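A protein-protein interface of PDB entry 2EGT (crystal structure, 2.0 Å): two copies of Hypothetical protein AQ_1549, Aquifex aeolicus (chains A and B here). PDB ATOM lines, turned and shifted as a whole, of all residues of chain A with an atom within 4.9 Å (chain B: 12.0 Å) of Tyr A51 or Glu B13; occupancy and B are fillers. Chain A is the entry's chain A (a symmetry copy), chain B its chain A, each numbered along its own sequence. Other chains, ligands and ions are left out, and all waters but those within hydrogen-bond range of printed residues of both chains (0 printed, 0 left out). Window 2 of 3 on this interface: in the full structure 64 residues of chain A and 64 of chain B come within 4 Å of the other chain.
Printed residues of chain A that touch a printed residue of chain B: Gly A47, Val A48, Tyr A51, His A52 and Ile A64. Among the printed residues, 14 pairs touch across the chains. Among the printed residues, no Asp or Glu carboxylate lies within 4 Å of a Lys or Arg side-chain nitrogen of the other chain.
No position is printed for both chains.
CE2 of Phe B16 touches C of Gly A47, at 3.4 Å. CG2 of Val A48 touches O of Ala B14, 3.5 Å away. Val A48 touches Phe B16 (N to CE2, 3.7 Å). Val A48 touches Gly B28. CD of Glu B29 touches CG1 of Val A48, 3.8 Å away. CE1 of Tyr A51 touches CD1 of Leu B10 (3.8 Å). Glu B13 touches Tyr A51. O of Ile A64 touches O of Leu B8, 3.9 Å away. Glu B9 touches Ile A64 (CA to O, 3.4 Å). Phe B16 touches Ile A64 (CE1 to O, 3.7 Å).
The backbone carbonyl oxygen (O) of Ile A64 lies within hydrogen-bond range of the backbone NH (N) of Leu B10 (3.4 Å). The side-chain carboxylate of Glu B29 sits at hydrogen-bond distance from a ring nitrogen (NE2) of His A52 (2.8 Å).
The backbone carbonyl oxygen (O) of Glu B9 is in hydrogen-bond range of the backbone NH (N) of Leu B17 (2.7 Å). OG1 of Thr B15 is in hydrogen-bond range of O of Glu B13 (2.9 Å). The side-chain carboxylate (OE1) of Glu B13 lies within salt-bridge range of the side-chain amino group (NZ) of Lys B30 (2.8 Å). O of Ala B14 sits at hydrogen-bond distance from N of Glu B29 (2.9 Å). O of Phe B16 is in hydrogen-bond range of OG of Ser B18 (3.3 Å). The backbone NH of Phe B16 is in hydrogen-bond range of the backbone carbonyl oxygen of Ala B27, 2.7 Å away.
Of the printed residues of chain B, Gly A47 touches Phe B16 (3.4 Å). Of chain B, only Ala B14, Phe B16, Gly B28 and Glu B29 come within 4 Å of Val A48. Tyr A51 touches just these residues of chain B: Leu B10, Glu B13 and Ala B14. Of the printed residues of chain B, His A52 touches Ala B14 and Glu B29. No residue of chain B comes within 4 Å of Ile A53. No residue of chain B comes within 4 Å of Leu A54. Lys A55 touches none of the printed residues of chain B. Of chain B, only Leu B8 (3.9 Å), Glu B9 (3.4 Å), Leu B10 (3.4 Å) and Phe B16 (3.7 Å) come within 4 Å of Ile A64. Of the printed residues of chain A, Glu B9 touches Ile A64 (3.4 Å). Glu B13 touches just one residue of chain A: Tyr A51. Printed residues of chain A within 4 Å of Gly B28: Val A48 (3.8 Å). The nearest printed residue of chain A that does not touch Glu B13 is His A52 (6.3 Å).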
ATOM      1  N   GLY A  47      -2.247  10.133 -23.673  1.00  0.00           N
ATOM      2  CA  GLY A  47      -1.329   9.548 -22.710  1.00  0.00           C
ATOM      3  C   GLY A  47      -0.521   8.401 -23.283  1.00  0.00           C
ATOM      4  O   GLY A  47       0.649   8.215 -22.941  1.00  0.00           O
ATOM      5  N   VAL A  48      -1.146   7.612 -24.148  1.00  0.00           N
ATOM      6  CA  VAL A  48      -0.452   6.493 -24.764  1.00  0.00           C
ATOM      7  C   VAL A  48       0.640   7.033 -25.690  1.00  0.00           C
ATOM      8  O   VAL A  48       1.757   6.515 -25.696  1.00  0.00           O
ATOM      9  CB  VAL A  48      -1.436   5.593 -25.545  1.00  0.00           C
ATOM     10  CG1 VAL A  48      -0.675   4.646 -26.462  1.00  0.00           C
ATOM     11  CG2 VAL A  48      -2.284   4.781 -24.547  1.00  0.00           C
ATOM     12  N   ASP A  49       0.322   8.074 -26.460  1.00  0.00           N
ATOM     13  CA  ASP A  49       1.310   8.677 -27.361  1.00  0.00           C
ATOM     14  C   ASP A  49       2.493   9.178 -26.552  1.00  0.00           C
ATOM     15  O   ASP A  49       3.646   8.914 -26.887  1.00  0.00           O
ATOM     16  CB  ASP A  49       0.748   9.890 -28.112  1.00  0.00           C
ATOM     17  CG  ASP A  49      -0.402   9.549 -29.039  1.00  0.00           C
ATOM     18  OD1 ASP A  49      -0.434   8.437 -29.602  1.00  0.00           O
ATOM     19  OD2 ASP A  49      -1.268  10.429 -29.224  1.00  0.00           O
ATOM     20  N   VAL A  50       2.194   9.929 -25.495  1.00  0.00           N
ATOM     21  CA  VAL A  50       3.226  10.505 -24.634  1.00  0.00           C
ATOM     22  C   VAL A  50       4.137   9.449 -24.034  1.00  0.00           C
ATOM     23  O   VAL A  50       5.357   9.603 -24.033  1.00  0.00           O
ATOM     24  CB  VAL A  50       2.594  11.341 -23.502  1.00  0.00           C
ATOM     25  CG1 VAL A  50       3.667  11.819 -22.537  1.00  0.00           C
ATOM     26  CG2 VAL A  50       1.846  12.522 -24.107  1.00  0.00           C
ATOM     27  N   TYR A  51       3.546   8.377 -23.517  1.00  0.00           N
ATOM     28  CA  TYR A  51       4.327   7.295 -22.935  1.00  0.00           C
ATOM     29  C   TYR A  51       5.277   6.697 -23.977  1.00  0.00           C
ATOM     30  O   TYR A  51       6.452   6.464 -23.693  1.00  0.00           O
ATOM     31  CB  TYR A  51       3.405   6.187 -22.414  1.00  0.00           C
ATOM     32  CG  TYR A  51       4.147   5.059 -21.732  1.00  0.00           C
ATOM     33  CD1 TYR A  51       4.389   5.087 -20.359  1.00  0.00           C
ATOM     34  CD2 TYR A  51       4.657   3.990 -22.468  1.00  0.00           C
ATOM     35  CE1 TYR A  51       5.124   4.082 -19.737  1.00  0.00           C
ATOM     36  CE2 TYR A  51       5.395   2.981 -21.859  1.00  0.00           C
ATOM     37  CZ  TYR A  51       5.626   3.033 -20.495  1.00  0.00           C
ATOM     38  OH  TYR A  51       6.364   2.042 -19.890  1.00  0.00           O
ATOM     39  N   HIS A  52       4.769   6.440 -25.180  1.00  0.00           N
ATOM     40  CA  HIS A  52       5.598   5.846 -26.232  1.00  0.00           C
ATOM     41  C   HIS A  52       6.700   6.772 -26.737  1.00  0.00           C
ATOM     42  O   HIS A  52       7.826   6.334 -26.978  1.00  0.00           O
ATOM     43  CB  HIS A  52       4.737   5.402 -27.418  1.00  0.00           C
ATOM     44  CG  HIS A  52       3.877   4.211 -27.128  1.00  0.00           C
ATOM     45  ND1 HIS A  52       4.325   3.129 -26.403  1.00  0.00           N
ATOM     46  CD2 HIS A  52       2.608   3.916 -27.499  1.00  0.00           C
ATOM     47  CE1 HIS A  52       3.369   2.218 -26.336  1.00  0.00           C
ATOM     48  NE2 HIS A  52       2.317   2.671 -26.994  1.00  0.00           N
ATOM     49  N   ILE A  53       6.379   8.047 -26.907  1.00  0.00           N
ATOM     50  CA  ILE A  53       7.373   8.994 -27.390  1.00  0.00           C
ATOM     51  C   ILE A  53       8.487   9.162 -26.354  1.00  0.00           C
ATOM     52  O   ILE A  53       9.672   9.191 -26.702  1.00  0.00           O
ATOM     53  CB  ILE A  53       6.719  10.357 -27.721  1.00  0.00           C
ATOM     54  CG1 ILE A  53       5.744  10.179 -28.890  1.00  0.00           C
ATOM     55  CG2 ILE A  53       7.797  11.385 -28.093  1.00  0.00           C
ATOM     56  CD1 ILE A  53       4.882  11.399 -29.187  1.00  0.00           C
ATOM     57  N   LEU A  54       8.113   9.259 -25.081  1.00  0.00           N
ATOM     58  CA  LEU A  54       9.100   9.412 -24.018  1.00  0.00           C
ATOM     59  C   LEU A  54      10.037   8.204 -23.938  1.00  0.00           C
ATOM     60  O   LEU A  54      11.247   8.357 -23.740  1.00  0.00           O
ATOM     61  CB  LEU A  54       8.405   9.618 -22.671  1.00  0.00           C
ATOM     62  CG  LEU A  54       7.707  10.968 -22.487  1.00  0.00           C
ATOM     63  CD1 LEU A  54       7.053  11.025 -21.106  1.00  0.00           C
ATOM     64  CD2 LEU A  54       8.731  12.095 -22.642  1.00  0.00           C
ATOM     65  N   LYS A  55       9.483   7.003 -24.080  1.00  0.00           N
ATOM     66  CA  LYS A  55      10.302   5.794 -24.033  1.00  0.00           C
ATOM     67  C   LYS A  55      11.226   5.754 -25.247  1.00  0.00           C
ATOM     68  O   LYS A  55      12.378   5.344 -25.142  1.00  0.00           O
ATOM     69  CB  LYS A  55       9.423   4.539 -24.013  1.00  0.00           C
ATOM     70  CG  LYS A  55       8.562   4.387 -22.765  1.00  0.00           C
ATOM     71  CD  LYS A  55       9.393   4.163 -21.504  1.00  0.00           C
ATOM     72  CE  LYS A  55      10.173   2.859 -21.577  1.00  0.00           C
ATOM     73  NZ  LYS A  55      10.827   2.525 -20.278  1.00  0.00           N
ATOM     74  N   VAL A  61      10.519   6.852 -17.427  1.00  0.00           N
ATOM     75  CA  VAL A  61       9.209   7.172 -16.872  1.00  0.00           C
ATOM     76  C   VAL A  61       8.786   6.320 -15.679  1.00  0.00           C
ATOM     77  O   VAL A  61       8.646   5.099 -15.791  1.00  0.00           O
ATOM     78  CB  VAL A  61       8.109   7.047 -17.950  1.00  0.00           C
ATOM     79  CG1 VAL A  61       6.754   7.427 -17.357  1.00  0.00           C
ATOM     80  CG2 VAL A  61       8.442   7.932 -19.140  1.00  0.00           C
ATOM     81  N   ILE A  64       3.005   8.829 -15.197  1.00  0.00           N
ATOM     82  CA  ILE A  64       2.484   9.902 -16.020  1.00  0.00           C
ATOM     83  C   ILE A  64       1.081  10.168 -15.506  1.00  0.00           C
ATOM     84  O   ILE A  64       0.236   9.271 -15.493  1.00  0.00           O
ATOM     85  CB  ILE A  64       2.393   9.515 -17.511  1.00  0.00           C
ATOM     86  CG1 ILE A  64       3.793   9.321 -18.095  1.00  0.00           C
ATOM     87  CG2 ILE A  64       1.647  10.603 -18.284  1.00  0.00           C
ATOM     88  CD1 ILE A  64       3.789   8.855 -19.537  1.00  0.00           C
ATOM     89  N   LEU B   8      -6.102  10.730 -14.835  1.00  0.00           N
ATOM     90  CA  LEU B   8      -5.479   9.478 -15.244  1.00  0.00           C
ATOM     91  C   LEU B   8      -4.076   9.336 -14.654  1.00  0.00           C
ATOM     92  O   LEU B   8      -3.361  10.327 -14.468  1.00  0.00           O
ATOM     93  CB  LEU B   8      -5.378   9.399 -16.772  1.00  0.00           C
ATOM     94  CG  LEU B   8      -6.631   9.113 -17.607  1.00  0.00           C
ATOM     95  CD1 LEU B   8      -7.693  10.167 -17.350  1.00  0.00           C
ATOM     96  CD2 LEU B   8      -6.254   9.091 -19.072  1.00  0.00           C
ATOM     97  N   GLU B   9      -3.701   8.100 -14.350  1.00  0.00           N
ATOM     98  CA  GLU B   9      -2.375   7.790 -13.833  1.00  0.00           C
ATOM     99  C   GLU B   9      -2.020   6.401 -14.351  1.00  0.00           C
ATOM    100  O   GLU B   9      -2.902   5.557 -14.518  1.00  0.00           O
ATOM    101  CB  GLU B   9      -2.359   7.797 -12.302  1.00  0.00           C
ATOM    102  CG  GLU B   9      -3.321   6.827 -11.658  1.00  0.00           C
ATOM    103  CD  GLU B   9      -3.111   6.726 -10.161  1.00  0.00           C
ATOM    104  OE1 GLU B   9      -2.876   7.775  -9.525  1.00  0.00           O
ATOM    105  OE2 GLU B   9      -3.191   5.601  -9.620  1.00  0.00           O
ATOM    106  N   LEU B  10      -0.740   6.157 -14.612  1.00  0.00           N
ATOM    107  CA  LEU B  10      -0.330   4.850 -15.118  1.00  0.00           C
ATOM    108  C   LEU B  10      -0.632   3.715 -14.149  1.00  0.00           C
ATOM    109  O   LEU B  10      -0.408   3.836 -12.943  1.00  0.00           O
ATOM    110  CB  LEU B  10       1.172   4.831 -15.433  1.00  0.00           C
ATOM    111  CG  LEU B  10       1.705   5.570 -16.664  1.00  0.00           C
ATOM    112  CD1 LEU B  10       3.220   5.408 -16.729  1.00  0.00           C
ATOM    113  CD2 LEU B  10       1.057   5.022 -17.929  1.00  0.00           C
ATOM    114  N   SER B  11      -1.150   2.614 -14.690  1.00  0.00           N
ATOM    115  CA  SER B  11      -1.433   1.421 -13.904  1.00  0.00           C
ATOM    116  C   SER B  11      -0.444   0.352 -14.388  1.00  0.00           C
ATOM    117  O   SER B  11      -0.145  -0.608 -13.679  1.00  0.00           O
ATOM    118  CB  SER B  11      -2.883   0.967 -14.106  1.00  0.00           C
ATOM    119  OG  SER B  11      -3.202   0.845 -15.477  1.00  0.00           O
ATOM    120  N   SER B  12       0.055   0.539 -15.608  1.00  0.00           N
ATOM    121  CA  SER B  12       1.046  -0.344 -16.220  1.00  0.00           C
ATOM    122  C   SER B  12       1.569   0.376 -17.461  1.00  0.00           C
ATOM    123  O   SER B  12       1.137   1.493 -17.753  1.00  0.00           O
ATOM    124  CB  SER B  12       0.440  -1.707 -16.602  1.00  0.00           C
ATOM    125  OG  SER B  12      -0.536  -1.586 -17.616  1.00  0.00           O
ATOM    126  N   GLU B  13       2.492  -0.247 -18.190  1.00  0.00           N
ATOM    127  CA  GLU B  13       3.059   0.387 -19.381  1.00  0.00           C
ATOM    128  C   GLU B  13       2.001   0.914 -20.354  1.00  0.00           C
ATOM    129  O   GLU B  13       1.149   0.162 -20.826  1.00  0.00           O
ATOM    130  CB  GLU B  13       3.989  -0.591 -20.114  1.00  0.00           C
ATOM    131  CG  GLU B  13       5.246  -0.961 -19.331  1.00  0.00           C
ATOM    132  CD  GLU B  13       5.106  -2.246 -18.536  1.00  0.00           C
ATOM    133  OE1 GLU B  13       3.965  -2.642 -18.209  1.00  0.00           O
ATOM    134  OE2 GLU B  13       6.149  -2.860 -18.224  1.00  0.00           O
ATOM    135  N   ALA B  14       2.067   2.215 -20.643  1.00  0.00           N
ATOM    136  CA  ALA B  14       1.141   2.872 -21.557  1.00  0.00           C
ATOM    137  C   ALA B  14      -0.325   2.551 -21.267  1.00  0.00           C
ATOM    138  O   ALA B  14      -1.156   2.521 -22.178  1.00  0.00           O
ATOM    139  CB  ALA B  14       1.477   2.491 -22.995  1.00  0.00           C
ATOM    140  N   THR B  15      -0.640   2.320 -20.001  1.00  0.00           N
ATOM    141  CA  THR B  15      -2.005   1.987 -19.608  1.00  0.00           C
ATOM    142  C   THR B  15      -2.383   2.837 -18.405  1.00  0.00           C
ATOM    143  O   THR B  15      -1.617   2.940 -17.444  1.00  0.00           O
ATOM    144  CB  THR B  15      -2.110   0.492 -19.275  1.00  0.00           C
ATOM    145  OG1 THR B  15      -1.660  -0.267 -20.409  1.00  0.00           O
ATOM    146  CG2 THR B  15      -3.550   0.109 -18.957  1.00  0.00           C
ATOM    147  N   PHE B  16      -3.573   3.426 -18.449  1.00  0.00           N
ATOM    148  CA  PHE B  16      -4.002   4.329 -17.387  1.00  0.00           C
ATOM    149  C   PHE B  16      -5.219   3.987 -16.547  1.00  0.00           C
ATOM    150  O   PHE B  16      -6.251   3.558 -17.065  1.00  0.00           O
ATOM    151  CB  PHE B  16      -4.245   5.710 -17.991  1.00  0.00           C
ATOM    152  CG  PHE B  16      -3.037   6.306 -18.651  1.00  0.00           C
ATOM    153  CD1 PHE B  16      -2.166   7.118 -17.931  1.00  0.00           C
ATOM    154  CD2 PHE B  16      -2.765   6.055 -19.990  1.00  0.00           C
ATOM    155  CE1 PHE B  16      -1.039   7.675 -18.539  1.00  0.00           C
ATOM    156  CE2 PHE B  16      -1.640   6.605 -20.606  1.00  0.00           C
ATOM    157  CZ  PHE B  16      -0.777   7.417 -19.873  1.00  0.00           C
ATOM    158  N   LEU B  17      -5.091   4.193 -15.239  1.00  0.00           N
ATOM    159  CA  LEU B  17      -6.220   4.011 -14.337  1.00  0.00           C
ATOM    160  C   LEU B  17      -6.886   5.363 -14.553  1.00  0.00           C
ATOM    161  O   LEU B  17      -6.270   6.404 -14.310  1.00  0.00           O
ATOM    162  CB  LEU B  17      -5.760   3.880 -12.884  1.00  0.00           C
ATOM    163  CG  LEU B  17      -6.906   3.893 -11.865  1.00  0.00           C
ATOM    164  CD1 LEU B  17      -7.862   2.736 -12.149  1.00  0.00           C
ATOM    165  CD2 LEU B  17      -6.343   3.796 -10.455  1.00  0.00           C
ATOM    166  N   SER B  18      -8.127   5.352 -15.023  1.00  0.00           N
ATOM    167  CA  SER B  18      -8.832   6.586 -15.339  1.00  0.00           C
ATOM    168  C   SER B  18      -9.978   6.829 -14.374  1.00  0.00           C
ATOM    169  O   SER B  18     -10.935   6.060 -14.327  1.00  0.00           O
ATOM    170  CB  SER B  18      -9.350   6.503 -16.777  1.00  0.00           C
ATOM    171  OG  SER B  18      -8.312   6.056 -17.642  1.00  0.00           O
ATOM    172  N   THR B  26      -9.907   1.205 -16.753  1.00  0.00           N
ATOM    173  CA  THR B  26      -8.530   1.157 -17.207  1.00  0.00           C
ATOM    174  C   THR B  26      -8.516   1.328 -18.719  1.00  0.00           C
ATOM    175  O   THR B  26      -9.184   0.585 -19.441  1.00  0.00           O
ATOM    176  CB  THR B  26      -7.872  -0.175 -16.800  1.00  0.00           C
ATOM    177  OG1 THR B  26      -7.913  -0.299 -15.373  1.00  0.00           O
ATOM    178  CG2 THR B  26      -6.421  -0.221 -17.257  1.00  0.00           C
ATOM    179  N   ALA B  27      -7.761   2.315 -19.193  1.00  0.00           N
ATOM    180  CA  ALA B  27      -7.682   2.596 -20.627  1.00  0.00           C
ATOM    181  C   ALA B  27      -6.242   2.756 -21.105  1.00  0.00           C
ATOM    182  O   ALA B  27      -5.397   3.308 -20.398  1.00  0.00           O
ATOM    183  CB  ALA B  27      -8.479   3.860 -20.956  1.00  0.00           C
ATOM    184  N   GLY B  28      -5.977   2.284 -22.320  1.00  0.00           N
ATOM    185  CA  GLY B  28      -4.639   2.373 -22.869  1.00  0.00           C
ATOM    186  C   GLY B  28      -4.262   1.089 -23.581  1.00  0.00           C
ATOM    187  O   GLY B  28      -5.130   0.295 -23.932  1.00  0.00           O
ATOM    188  N   GLU B  29      -2.966   0.874 -23.775  1.00  0.00           N
ATOM    189  CA  GLU B  29      -2.482  -0.309 -24.475  1.00  0.00           C
ATOM    190  C   GLU B  29      -2.910  -1.629 -23.846  1.00  0.00           C
ATOM    191  O   GLU B  29      -3.225  -2.579 -24.560  1.00  0.00           O
ATOM    192  CB  GLU B  29      -0.956  -0.256 -24.596  1.00  0.00           C
ATOM    193  CG  GLU B  29      -0.446   0.935 -25.398  1.00  0.00           C
ATOM    194  CD  GLU B  29      -0.754   0.834 -26.886  1.00  0.00           C
ATOM    195  OE1 GLU B  29      -1.937   0.677 -27.253  1.00  0.00           O
ATOM    196  OE2 GLU B  29       0.194   0.921 -27.692  1.00  0.00           O
ATOM    197  N   LYS B  30      -2.927  -1.696 -22.519  1.00  0.00           N
ATOM    198  CA  LYS B  30      -3.329  -2.923 -21.839  1.00  0.00           C
ATOM    199  C   LYS B  30      -4.672  -2.755 -21.142  1.00  0.00           C
ATOM    200  O   LYS B  30      -4.947  -3.412 -20.141  1.00  0.00           O
ATOM    201  CB  LYS B  30      -2.277  -3.338 -20.811  1.00  0.00           C
ATOM    202  CG  LYS B  30      -0.914  -3.673 -21.394  1.00  0.00           C
ATOM    203  CD  LYS B  30       0.068  -3.907 -20.258  1.00  0.00           C
ATOM    204  CE  LYS B  30       1.456  -4.238 -20.749  1.00  0.00           C
ATOM    205  NZ  LYS B  30       2.355  -4.420 -19.576  1.00  0.00           N
ATOM    206  N   GLY B  31      -5.500  -1.859 -21.670  1.00  0.00           N
ATOM    207  CA  GLY B  31      -6.812  -1.630 -21.095  1.00  0.00           C
ATOM    208  C   GLY B  31      -7.793  -1.421 -22.230  1.00  0.00           C
ATOM    209  O   GLY B  31      -7.536  -1.849 -23.356  1.00  0.00           O
ATOM    210  N   LEU B  32      -8.915  -0.771 -21.944  1.00  0.00           N
ATOM    211  CA  LEU B  32      -9.901  -0.504 -22.976  1.00  0.00           C
ATOM    212  C   LEU B  32      -9.255   0.416 -24.013  1.00  0.00           C
ATOM    213  O   LEU B  32      -8.420   1.255 -23.672  1.00  0.00           O
ATOM    214  CB  LEU B  32     -11.137   0.151 -22.355  1.00  0.00           C
ATOM    215  CG  LEU B  32     -11.880  -0.749 -21.365  1.00  0.00           C
ATOM    216  CD1 LEU B  32     -12.910   0.053 -20.594  1.00  0.00           C
ATOM    217  CD2 LEU B  32     -12.542  -1.897 -22.119  1.00  0.00           C
ATOM    218  N   ASN B  33      -9.629   0.244 -25.278  1.00  0.00           N
ATOM    219  CA  ASN B  33      -9.066   1.048 -26.357  1.00  0.00           C
ATOM    220  C   ASN B  33      -9.672   2.447 -26.370  1.00  0.00           C
ATOM    221  O   ASN B  33     -10.890   2.604 -26.339  1.00  0.00           O
ATOM    222  CB  ASN B  33      -9.302   0.352 -27.702  1.00  0.00           C
ATOM    223  CG  ASN B  33      -8.754   1.143 -28.868  1.00  0.00           C
ATOM    224  OD1 ASN B  33      -9.475   1.901 -29.512  1.00  0.00           O
ATOM    225  ND2 ASN B  33      -7.465   0.978 -29.142  1.00  0.00           N
ATOM    226  N   PRO B  34      -8.822   3.483 -26.408  1.00  0.00           N
ATOM    227  CA  PRO B  34      -9.308   4.864 -26.418  1.00  0.00           C
ATOM    228  C   PRO B  34     -10.294   5.198 -27.535  1.00  0.00           C
ATOM    229  O   PRO B  34     -11.303   5.849 -27.290  1.00  0.00           O
ATOM    230  CB  PRO B  34      -8.019   5.678 -26.494  1.00  0.00           C
ATOM    231  CG  PRO B  34      -7.062   4.830 -25.696  1.00  0.00           C
ATOM    232  CD  PRO B  34      -7.356   3.447 -26.248  1.00  0.00           C
